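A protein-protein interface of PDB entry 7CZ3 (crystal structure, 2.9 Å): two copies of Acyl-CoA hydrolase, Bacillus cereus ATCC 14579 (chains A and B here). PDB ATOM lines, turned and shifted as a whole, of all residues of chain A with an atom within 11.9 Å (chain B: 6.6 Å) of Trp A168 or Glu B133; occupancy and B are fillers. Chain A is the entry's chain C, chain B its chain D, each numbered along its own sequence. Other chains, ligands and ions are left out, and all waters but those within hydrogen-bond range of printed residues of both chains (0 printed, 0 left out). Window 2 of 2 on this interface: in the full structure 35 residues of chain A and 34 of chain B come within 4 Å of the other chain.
The backbone carbonyl oxygen of Phe B78 sits at hydrogen-bond distance from the backbone NH of Phe B90 (2.7 Å).
Among the printed residues, pairs that only touch across the chains: Trp A168 with Glu B133, Trp A168 with Trp B136, Trp A168 with Gln B132, Met A158 with Phe B90, Asn A169 with Trp B136, Leu A162 with Lys B92, Pro A167 with Gln B132 and Leu A162 with Glu B133.
Trp A168 touches just these residues of chain B: Gln B132, Glu B133 and Trp B136.
Of chain A, only Leu A162 and Trp A168 come within 4 Å of Glu B133.
Of chain A, only Trp A168 (3.6 Å) and Asn A169 (3.8 Å) come within 4 Å of Trp B136.
No residue of chain A comes within 4 Å of Leu B137.
Of the printed residues of chain A, Phe B90 touches Met A158.
Of the printed residues of chain B, Pro A167 touches Gln B132.
Printed residues of chain B within 4 Å of Asn A169: Trp B136 (3.8 Å).
Printed residues of chain B within 4 Å of Leu A162: Lys B92 and Glu B133.
His B135 touches none of the printed residues of chain A.
The nearest printed residue of chain B that does not touch Leu A162 is Phe B90 (4.5 Å).
Of the 13 printed residues of chain B, 5 touch a printed residue of chain A.
Printed residues of chain B that touch a printed residue of chain A: Phe B90, Lys B92, Gln B132, Glu B133 and Trp B136.
Hydrophobic or aromatic side chains of chain B that line the printed part of chain A: Phe B90 and Trp B136.
Of the 16 printed residues of chain A, 5 touch a printed residue of chain B.
Among the printed residues, no Asp or Glu carboxylate lies within 4 Å of a Lys or Arg side-chain nitrogen of the other chain.
No position is printed for both chains.
Of the 8 pairs that touch across the chains among the printed residues, none has its exchanged pair printed and touching as well.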
ATOM      1  N   LYS A 154      14.710  19.000 -35.368  1.00  0.00           N
ATOM      2  CA  LYS A 154      15.177  18.150 -34.247  1.00  0.00           C
ATOM      3  C   LYS A 154      16.377  17.339 -34.732  1.00  0.00           C
ATOM      4  O   LYS A 154      17.436  17.410 -34.104  1.00  0.00           O
ATOM      5  CB  LYS A 154      14.087  17.156 -33.843  1.00  0.00           C
ATOM      6  CG  LYS A 154      13.029  17.664 -32.877  1.00  0.00           C
ATOM      7  CD  LYS A 154      12.087  16.569 -32.424  1.00  0.00           C
ATOM      8  CE  LYS A 154      11.223  16.957 -31.243  1.00  0.00           C
ATOM      9  NZ  LYS A 154      10.262  15.888 -30.874  1.00  0.00           N
ATOM     10  N   SER A 155      16.226  16.670 -35.874  1.00  0.00           N
ATOM     11  CA  SER A 155      17.304  15.795 -36.386  1.00  0.00           C
ATOM     12  C   SER A 155      18.559  16.628 -36.598  1.00  0.00           C
ATOM     13  O   SER A 155      19.611  16.226 -36.110  1.00  0.00           O
ATOM     14  CB  SER A 155      16.883  15.176 -37.679  1.00  0.00           C
ATOM     15  OG  SER A 155      15.696  14.429 -37.513  1.00  0.00           O
ATOM     16  N   LYS A 156      18.426  17.755 -37.288  1.00  0.00           N
ATOM     17  CA  LYS A 156      19.585  18.640 -37.535  1.00  0.00           C
ATOM     18  C   LYS A 156      20.098  19.108 -36.178  1.00  0.00           C
ATOM     19  O   LYS A 156      21.313  19.175 -35.993  1.00  0.00           O
ATOM     20  CB  LYS A 156      19.127  19.834 -38.365  1.00  0.00           C
ATOM     21  CG  LYS A 156      20.038  20.229 -39.512  1.00  0.00           C
ATOM     22  CD  LYS A 156      19.252  20.802 -40.662  1.00  0.00           C
ATOM     23  CE  LYS A 156      20.064  21.692 -41.573  1.00  0.00           C
ATOM     24  NZ  LYS A 156      21.266  20.994 -42.083  1.00  0.00           N
ATOM     25  N   GLU A 157      19.186  19.397 -35.257  1.00  0.00           N
ATOM     26  CA  GLU A 157      19.612  19.842 -33.913  1.00  0.00           C
ATOM     27  C   GLU A 157      20.365  18.706 -33.228  1.00  0.00           C
ATOM     28  O   GLU A 157      21.405  18.970 -32.645  1.00  0.00           O
ATOM     29  CB  GLU A 157      18.396  20.211 -33.073  1.00  0.00           C
ATOM     30  CG  GLU A 157      17.702  21.466 -33.556  1.00  0.00           C
ATOM     31  CD  GLU A 157      16.639  22.007 -32.620  1.00  0.00           C
ATOM     32  OE1 GLU A 157      16.343  21.336 -31.622  1.00  0.00           O
ATOM     33  OE2 GLU A 157      16.117  23.097 -32.893  1.00  0.00           O
ATOM     34  N   MET A 158      19.875  17.479 -33.350  1.00  0.00           N
ATOM     35  CA  MET A 158      20.537  16.347 -32.654  1.00  0.00           C
ATOM     36  C   MET A 158      21.938  16.110 -33.217  1.00  0.00           C
ATOM     37  O   MET A 158      22.781  15.601 -32.488  1.00  0.00           O
ATOM     38  CB  MET A 158      19.724  15.064 -32.776  1.00  0.00           C
ATOM     39  CG  MET A 158      20.260  13.981 -31.906  1.00  0.00           C
ATOM     40  SD  MET A 158      18.880  13.140 -31.169  1.00  0.00           S
ATOM     41  CE  MET A 158      19.694  12.363 -29.776  1.00  0.00           C
ATOM     42  N   ALA A 159      22.126  16.383 -34.499  1.00  0.00           N
ATOM     43  CA  ALA A 159      23.446  16.264 -35.164  1.00  0.00           C
ATOM     44  C   ALA A 159      24.515  17.035 -34.365  1.00  0.00           C
ATOM     45  O   ALA A 159      25.516  16.401 -33.933  1.00  0.00           O
ATOM     46  CB  ALA A 159      23.355  16.764 -36.584  1.00  0.00           C
ATOM     47  N   GLU A 160      24.293  18.342 -34.154  1.00  0.00           N
ATOM     48  CA  GLU A 160      25.205  19.278 -33.432  1.00  0.00           C
ATOM     49  C   GLU A 160      25.425  18.813 -31.976  1.00  0.00           C
ATOM     50  O   GLU A 160      26.595  18.909 -31.497  1.00  0.00           O
ATOM     51  CB  GLU A 160      24.638  20.699 -33.508  1.00  0.00           C
ATOM     52  CG  GLU A 160      24.414  21.207 -34.925  1.00  0.00           C
ATOM     53  CD  GLU A 160      25.575  20.976 -35.885  1.00  0.00           C
ATOM     54  OE1 GLU A 160      25.835  19.799 -36.239  1.00  0.00           O
ATOM     55  OE2 GLU A 160      26.224  21.975 -36.280  1.00  0.00           O
ATOM     56  N   VAL A 161      24.376  18.327 -31.289  1.00  0.00           N
ATOM     57  CA  VAL A 161      24.489  17.754 -29.907  1.00  0.00           C
ATOM     58  C   VAL A 161      25.547  16.626 -29.921  1.00  0.00           C
ATOM     59  O   VAL A 161      26.366  16.555 -28.974  1.00  0.00           O
ATOM     60  CB  VAL A 161      23.119  17.301 -29.326  1.00  0.00           C
ATOM     61  CG1 VAL A 161      23.212  16.526 -28.001  1.00  0.00           C
ATOM     62  CG2 VAL A 161      22.156  18.468 -29.152  1.00  0.00           C
ATOM     63  N   LEU A 162      25.501  15.770 -30.936  1.00  0.00           N
ATOM     64  CA  LEU A 162      26.441  14.627 -31.029  1.00  0.00           C
ATOM     65  C   LEU A 162      27.760  15.126 -31.610  1.00  0.00           C
ATOM     66  O   LEU A 162      28.808  14.651 -31.173  1.00  0.00           O
ATOM     67  CB  LEU A 162      25.817  13.554 -31.920  1.00  0.00           C
ATOM     68  CG  LEU A 162      24.642  12.794 -31.316  1.00  0.00           C
ATOM     69  CD1 LEU A 162      24.031  11.873 -32.345  1.00  0.00           C
ATOM     70  CD2 LEU A 162      25.070  12.001 -30.099  1.00  0.00           C
ATOM     71  N   THR A 163      27.685  15.999 -32.613  1.00  0.00           N
ATOM     72  CA  THR A 163      28.891  16.542 -33.288  1.00  0.00           C
ATOM     73  C   THR A 163      29.696  17.416 -32.329  1.00  0.00           C
ATOM     74  O   THR A 163      30.837  17.051 -32.033  1.00  0.00           O
ATOM     75  CB  THR A 163      28.502  17.498 -34.414  1.00  0.00           C
ATOM     76  OG1 THR A 163      27.623  16.801 -35.289  1.00  0.00           O
ATOM     77  CG2 THR A 163      29.696  18.004 -35.188  1.00  0.00           C
ATOM     78  N   LEU A 164      29.086  18.554 -31.976  1.00  0.00           N
ATOM     79  CA  LEU A 164      29.644  19.663 -31.166  1.00  0.00           C
ATOM     80  C   LEU A 164      29.635  19.347 -29.678  1.00  0.00           C
ATOM     81  O   LEU A 164      30.002  20.228 -28.925  1.00  0.00           O
ATOM     82  CB  LEU A 164      28.758  20.885 -31.401  1.00  0.00           C
ATOM     83  CG  LEU A 164      28.844  21.523 -32.784  1.00  0.00           C
ATOM     84  CD1 LEU A 164      28.399  22.973 -32.728  1.00  0.00           C
ATOM     85  CD2 LEU A 164      30.252  21.430 -33.336  1.00  0.00           C
ATOM     86  N   SER A 165      29.035  18.211 -29.339  1.00  0.00           N
ATOM     87  CA  SER A 165      28.871  17.698 -27.957  1.00  0.00           C
ATOM     88  C   SER A 165      28.039  18.633 -27.079  1.00  0.00           C
ATOM     89  O   SER A 165      28.194  18.551 -25.862  1.00  0.00           O
ATOM     90  CB  SER A 165      30.176  17.423 -27.309  1.00  0.00           C
ATOM     91  OG  SER A 165      29.953  17.229 -25.925  1.00  0.00           O
ATOM     92  N   LYS A 166      27.268  19.525 -27.707  1.00  0.00           N
ATOM     93  CA  LYS A 166      26.416  20.505 -26.993  1.00  0.00           C
ATOM     94  C   LYS A 166      25.640  19.735 -25.932  1.00  0.00           C
ATOM     95  O   LYS A 166      24.924  18.815 -26.302  1.00  0.00           O
ATOM     96  CB  LYS A 166      25.545  21.253 -28.002  1.00  0.00           C
ATOM     97  CG  LYS A 166      26.336  22.159 -28.935  1.00  0.00           C
ATOM     98  CD  LYS A 166      25.766  22.333 -30.318  1.00  0.00           C
ATOM     99  CE  LYS A 166      24.640  23.338 -30.393  1.00  0.00           C
ATOM    100  NZ  LYS A 166      23.317  22.693 -30.234  1.00  0.00           N
ATOM    101  N   PRO A 167      25.752  20.079 -24.636  1.00  0.00           N
ATOM    102  CA  PRO A 167      25.129  19.294 -23.588  1.00  0.00           C
ATOM    103  C   PRO A 167      23.626  19.167 -23.817  1.00  0.00           C
ATOM    104  O   PRO A 167      22.969  20.108 -24.176  1.00  0.00           O
ATOM    105  CB  PRO A 167      25.427  20.054 -22.296  1.00  0.00           C
ATOM    106  CG  PRO A 167      25.819  21.429 -22.764  1.00  0.00           C
ATOM    107  CD  PRO A 167      26.467  21.232 -24.116  1.00  0.00           C
ATOM    108  N   TRP A 168      23.159  17.946 -23.627  1.00  0.00           N
ATOM    109  CA  TRP A 168      21.744  17.581 -23.833  1.00  0.00           C
ATOM    110  C   TRP A 168      20.820  18.575 -23.138  1.00  0.00           C
ATOM    111  O   TRP A 168      21.028  18.817 -21.936  1.00  0.00           O
ATOM    112  CB  TRP A 168      21.569  16.133 -23.387  1.00  0.00           C
ATOM    113  CG  TRP A 168      22.556  15.314 -24.154  1.00  0.00           C
ATOM    114  CD1 TRP A 168      23.910  15.336 -24.015  1.00  0.00           C
ATOM    115  CD2 TRP A 168      22.285  14.466 -25.278  1.00  0.00           C
ATOM    116  NE1 TRP A 168      24.495  14.514 -24.935  1.00  0.00           N
ATOM    117  CE2 TRP A 168      23.521  13.970 -25.724  1.00  0.00           C
ATOM    118  CE3 TRP A 168      21.118  14.049 -25.921  1.00  0.00           C
ATOM    119  CZ2 TRP A 168      23.623  13.075 -26.783  1.00  0.00           C
ATOM    120  CZ3 TRP A 168      21.218  13.167 -26.971  1.00  0.00           C
ATOM    121  CH2 TRP A 168      22.455  12.690 -27.396  1.00  0.00           C
ATOM    122  N   ASN A 169      19.922  19.124 -23.966  1.00  0.00           N
ATOM    123  CA  ASN A 169      18.781  20.084 -23.815  1.00  0.00           C
ATOM    124  C   ASN A 169      19.049  21.290 -24.720  1.00  0.00           C
ATOM    125  O   ASN A 169      20.161  21.822 -24.616  1.00  0.00           O
ATOM    126  CB  ASN A 169      18.388  20.515 -22.397  1.00  0.00           C
ATOM    127  CG  ASN A 169      17.781  19.388 -21.589  1.00  0.00           C
ATOM    128  OD1 ASN A 169      16.592  19.109 -21.703  1.00  0.00           O
ATOM    129  ND2 ASN A 169      18.584  18.738 -20.768  1.00  0.00           N
ATOM    130  N   MET B   6      21.646  -0.263 -20.643  1.00  0.00           N
ATOM    131  CA  MET B   6      21.506   0.033 -22.096  1.00  0.00           C
ATOM    132  C   MET B   6      22.689  -0.543 -22.864  1.00  0.00           C
ATOM    133  O   MET B   6      22.458  -1.109 -23.952  1.00  0.00           O
ATOM    134  CB  MET B   6      21.488   1.532 -22.367  1.00  0.00           C
ATOM    135  CG  MET B   6      20.138   2.115 -22.173  1.00  0.00           C
ATOM    136  SD  MET B   6      20.204   3.892 -22.361  1.00  0.00           S
ATOM    137  CE  MET B   6      18.548   4.257 -21.790  1.00  0.00           C
ATOM    138  N   PHE B  78      21.785   0.990 -29.743  1.00  0.00           N
ATOM    139  CA  PHE B  78      21.343   0.460 -28.428  1.00  0.00           C
ATOM    140  C   PHE B  78      19.839   0.706 -28.250  1.00  0.00           C
ATOM    141  O   PHE B  78      19.263   1.640 -28.856  1.00  0.00           O
ATOM    142  CB  PHE B  78      22.205   0.993 -27.278  1.00  0.00           C
ATOM    143  CG  PHE B  78      22.135   2.480 -27.038  1.00  0.00           C
ATOM    144  CD1 PHE B  78      22.870   3.367 -27.811  1.00  0.00           C
ATOM    145  CD2 PHE B  78      21.343   3.000 -26.023  1.00  0.00           C
ATOM    146  CE1 PHE B  78      22.804   4.736 -27.590  1.00  0.00           C
ATOM    147  CE2 PHE B  78      21.277   4.371 -25.803  1.00  0.00           C
ATOM    148  CZ  PHE B  78      22.005   5.237 -26.588  1.00  0.00           C
ATOM    149  N   PHE B  90      17.779   3.301 -30.298  1.00  0.00           N
ATOM    150  CA  PHE B  90      18.484   4.511 -30.794  1.00  0.00           C
ATOM    151  C   PHE B  90      19.616   4.035 -31.699  1.00  0.00           C
ATOM    152  O   PHE B  90      20.361   3.106 -31.304  1.00  0.00           O
ATOM    153  CB  PHE B  90      19.035   5.429 -29.694  1.00  0.00           C
ATOM    154  CG  PHE B  90      19.584   6.716 -30.260  1.00  0.00           C
ATOM    155  CD1 PHE B  90      18.849   7.471 -31.157  1.00  0.00           C
ATOM    156  CD2 PHE B  90      20.843   7.155 -29.937  1.00  0.00           C
ATOM    157  CE1 PHE B  90      19.359   8.635 -31.717  1.00  0.00           C
ATOM    158  CE2 PHE B  90      21.368   8.302 -30.515  1.00  0.00           C
ATOM    159  CZ  PHE B  90      20.627   9.046 -31.400  1.00  0.00           C
ATOM    160  N   LYS B  92      22.598   5.623 -34.289  1.00  0.00           N
ATOM    161  CA  LYS B  92      23.464   6.739 -34.734  1.00  0.00           C
ATOM    162  C   LYS B  92      24.256   6.266 -35.958  1.00  0.00           C
ATOM    163  O   LYS B  92      24.789   5.126 -35.904  1.00  0.00           O
ATOM    164  CB  LYS B  92      24.344   7.129 -33.546  1.00  0.00           C
ATOM    165  CG  LYS B  92      25.165   8.399 -33.701  1.00  0.00           C
ATOM    166  CD  LYS B  92      26.463   8.354 -32.906  1.00  0.00           C
ATOM    167  CE  LYS B  92      26.321   7.801 -31.499  1.00  0.00           C
ATOM    168  NZ  LYS B  92      27.651   7.519 -30.906  1.00  0.00           N
ATOM    169  N   PRO B 129      19.720   3.725 -18.024  1.00  0.00           N
ATOM    170  CA  PRO B 129      20.767   4.590 -18.553  1.00  0.00           C
ATOM    171  C   PRO B 129      21.916   4.795 -17.563  1.00  0.00           C
ATOM    172  O   PRO B 129      21.757   4.479 -16.419  1.00  0.00           O
ATOM    173  CB  PRO B 129      20.053   5.930 -18.735  1.00  0.00           C
ATOM    174  CG  PRO B 129      18.990   5.912 -17.675  1.00  0.00           C
ATOM    175  CD  PRO B 129      18.544   4.471 -17.603  1.00  0.00           C
ATOM    176  N   THR B 131      24.525   7.324 -18.881  1.00  0.00           N
ATOM    177  CA  THR B 131      25.257   8.486 -19.436  1.00  0.00           C
ATOM    178  C   THR B 131      24.296   9.630 -19.733  1.00  0.00           C
ATOM    179  O   THR B 131      23.094   9.366 -19.803  1.00  0.00           O
ATOM    180  CB  THR B 131      26.032   8.086 -20.695  1.00  0.00           C
ATOM    181  OG1 THR B 131      26.523   6.762 -20.502  1.00  0.00           O
ATOM    182  CG2 THR B 131      27.206   8.988 -20.993  1.00  0.00           C
ATOM    183  N   GLN B 132      24.838  10.848 -19.803  1.00  0.00           N
ATOM    184  CA  GLN B 132      24.104  12.094 -20.121  1.00  0.00           C
ATOM    185  C   GLN B 132      23.124  11.788 -21.245  1.00  0.00           C
ATOM    186  O   GLN B 132      21.914  11.883 -21.026  1.00  0.00           O
ATOM    187  CB  GLN B 132      25.087  13.092 -20.727  1.00  0.00           C
ATOM    188  CG  GLN B 132      25.542  14.195 -19.788  1.00  0.00           C
ATOM    189  CD  GLN B 132      26.197  15.311 -20.564  1.00  0.00           C
ATOM    190  OE1 GLN B 132      27.364  15.235 -20.942  1.00  0.00           O
ATOM    191  NE2 GLN B 132      25.435  16.356 -20.827  1.00  0.00           N
ATOM    192  N   GLU B 133      23.671  11.384 -22.387  1.00  0.00           N
ATOM    193  CA  GLU B 133      22.890  11.052 -23.603  1.00  0.00           C
ATOM    194  C   GLU B 133      21.902   9.928 -23.294  1.00  0.00           C
ATOM    195  O   GLU B 133      20.754  10.015 -23.732  1.00  0.00           O
ATOM    196  CB  GLU B 133      23.874  10.618 -24.686  1.00  0.00           C
ATOM    197  CG  GLU B 133      23.271   9.722 -25.744  1.00  0.00           C
ATOM    198  CD  GLU B 133      24.310   9.096 -26.654  1.00  0.00           C
ATOM    199  OE1 GLU B 133      24.071   7.987 -27.155  1.00  0.00           O
ATOM    200  OE2 GLU B 133      25.361   9.721 -26.850  1.00  0.00           O
ATOM    201  N   GLU B 134      22.334   8.930 -22.533  1.00  0.00           N
ATOM    202  CA  GLU B 134      21.444   7.789 -22.228  1.00  0.00           C
ATOM    203  C   GLU B 134      20.276   8.282 -21.376  1.00  0.00           C
ATOM    204  O   GLU B 134      19.147   7.863 -21.625  1.00  0.00           O
ATOM    205  CB  GLU B 134      22.226   6.701 -21.496  1.00  0.00           C
ATOM    206  CG  GLU B 134      23.569   6.399 -22.126  1.00  0.00           C
ATOM    207  CD  GLU B 134      24.142   5.019 -21.851  1.00  0.00           C
ATOM    208  OE1 GLU B 134      23.443   4.188 -21.261  1.00  0.00           O
ATOM    209  OE2 GLU B 134      25.293   4.783 -22.232  1.00  0.00           O
ATOM    210  N   HIS B 135      20.543   9.193 -20.445  1.00  0.00           N
ATOM    211  CA  HIS B 135      19.482   9.645 -19.502  1.00  0.00           C
ATOM    212  C   HIS B 135      18.410  10.452 -20.257  1.00  0.00           C
ATOM    213  O   HIS B 135      17.223  10.145 -20.046  1.00  0.00           O
ATOM    214  CB  HIS B 135      20.099  10.397 -18.308  1.00  0.00           C
ATOM    215  CG  HIS B 135      20.441   9.544 -17.123  1.00  0.00           C
ATOM    216  ND1 HIS B 135      19.474   8.912 -16.348  1.00  0.00           N
ATOM    217  CD2 HIS B 135      21.631   9.268 -16.539  1.00  0.00           C
ATOM    218  CE1 HIS B 135      20.061   8.262 -15.357  1.00  0.00           C
ATOM    219  NE2 HIS B 135      21.387   8.461 -15.455  1.00  0.00           N
ATOM    220  N   TRP B 136      18.814  11.410 -21.111  1.00  0.00           N
ATOM    221  CA  TRP B 136      17.953  12.198 -22.050  1.00  0.00           C
ATOM    222  C   TRP B 136      17.095  11.278 -22.940  1.00  0.00           C
ATOM    223  O   TRP B 136      15.994  11.701 -23.321  1.00  0.00           O
ATOM    224  CB  TRP B 136      18.810  13.128 -22.921  1.00  0.00           C
ATOM    225  CG  TRP B 136      18.051  14.206 -23.640  1.00  0.00           C
ATOM    226  CD1 TRP B 136      18.001  15.528 -23.292  1.00  0.00           C
ATOM    227  CD2 TRP B 136      17.270  14.093 -24.847  1.00  0.00           C
ATOM    228  NE1 TRP B 136      17.237  16.236 -24.182  1.00  0.00           N
ATOM    229  CE2 TRP B 136      16.767  15.381 -25.142  1.00  0.00           C
ATOM    230  CE3 TRP B 136      16.935  13.039 -25.706  1.00  0.00           C
ATOM    231  CZ2 TRP B 136      15.954  15.636 -26.245  1.00  0.00           C
ATOM    232  CZ3 TRP B 136      16.131  13.292 -26.798  1.00  0.00           C
ATOM    233  CH2 TRP B 136      15.648  14.573 -27.062  1.00  0.00           C
ATOM    234  N   LEU B 137      17.625  10.116 -23.307  1.00  0.00           N
ATOM    235  CA  LEU B 137      16.859   9.173 -24.154  1.00  0.00           C
ATOM    236  C   LEU B 137      15.718   8.617 -23.310  1.00  0.00           C
ATOM    237  O   LEU B 137      14.561   8.725 -23.730  1.00  0.00           O
ATOM    238  CB  LEU B 137      17.794   8.048 -24.597  1.00  0.00           C
ATOM    239  CG  LEU B 137      18.944   8.470 -25.502  1.00  0.00           C
ATOM    240  CD1 LEU B 137      19.742   7.260 -25.945  1.00  0.00           C
ATOM    241  CD2 LEU B 137      18.423   9.216 -26.711  1.00  0.00           C
ATOM    242  N   HIS B 138      16.061   8.021 -22.171  1.00  0.00           N
ATOM    243  CA  HIS B 138      15.043   7.428 -21.275  1.00  0.00           C
ATOM    244  C   HIS B 138      13.995   8.480 -20.942  1.00  0.00           C
ATOM    245  O   HIS B 138      12.827   8.269 -21.275  1.00  0.00           O
ATOM    246  CB  HIS B 138      15.696   6.937 -19.989  1.00  0.00           C
ATOM    247  CG  HIS B 138      14.930   5.835 -19.347  1.00  0.00           C
ATOM    248  ND1 HIS B 138      14.360   5.963 -18.104  1.00  0.00           N
ATOM    249  CD2 HIS B 138      14.625   4.596 -19.781  1.00  0.00           C
ATOM    250  CE1 HIS B 138      13.745   4.843 -17.790  1.00  0.00           C
ATOM    251  NE2 HIS B 138      13.894   3.987 -18.803  1.00  0.00           N
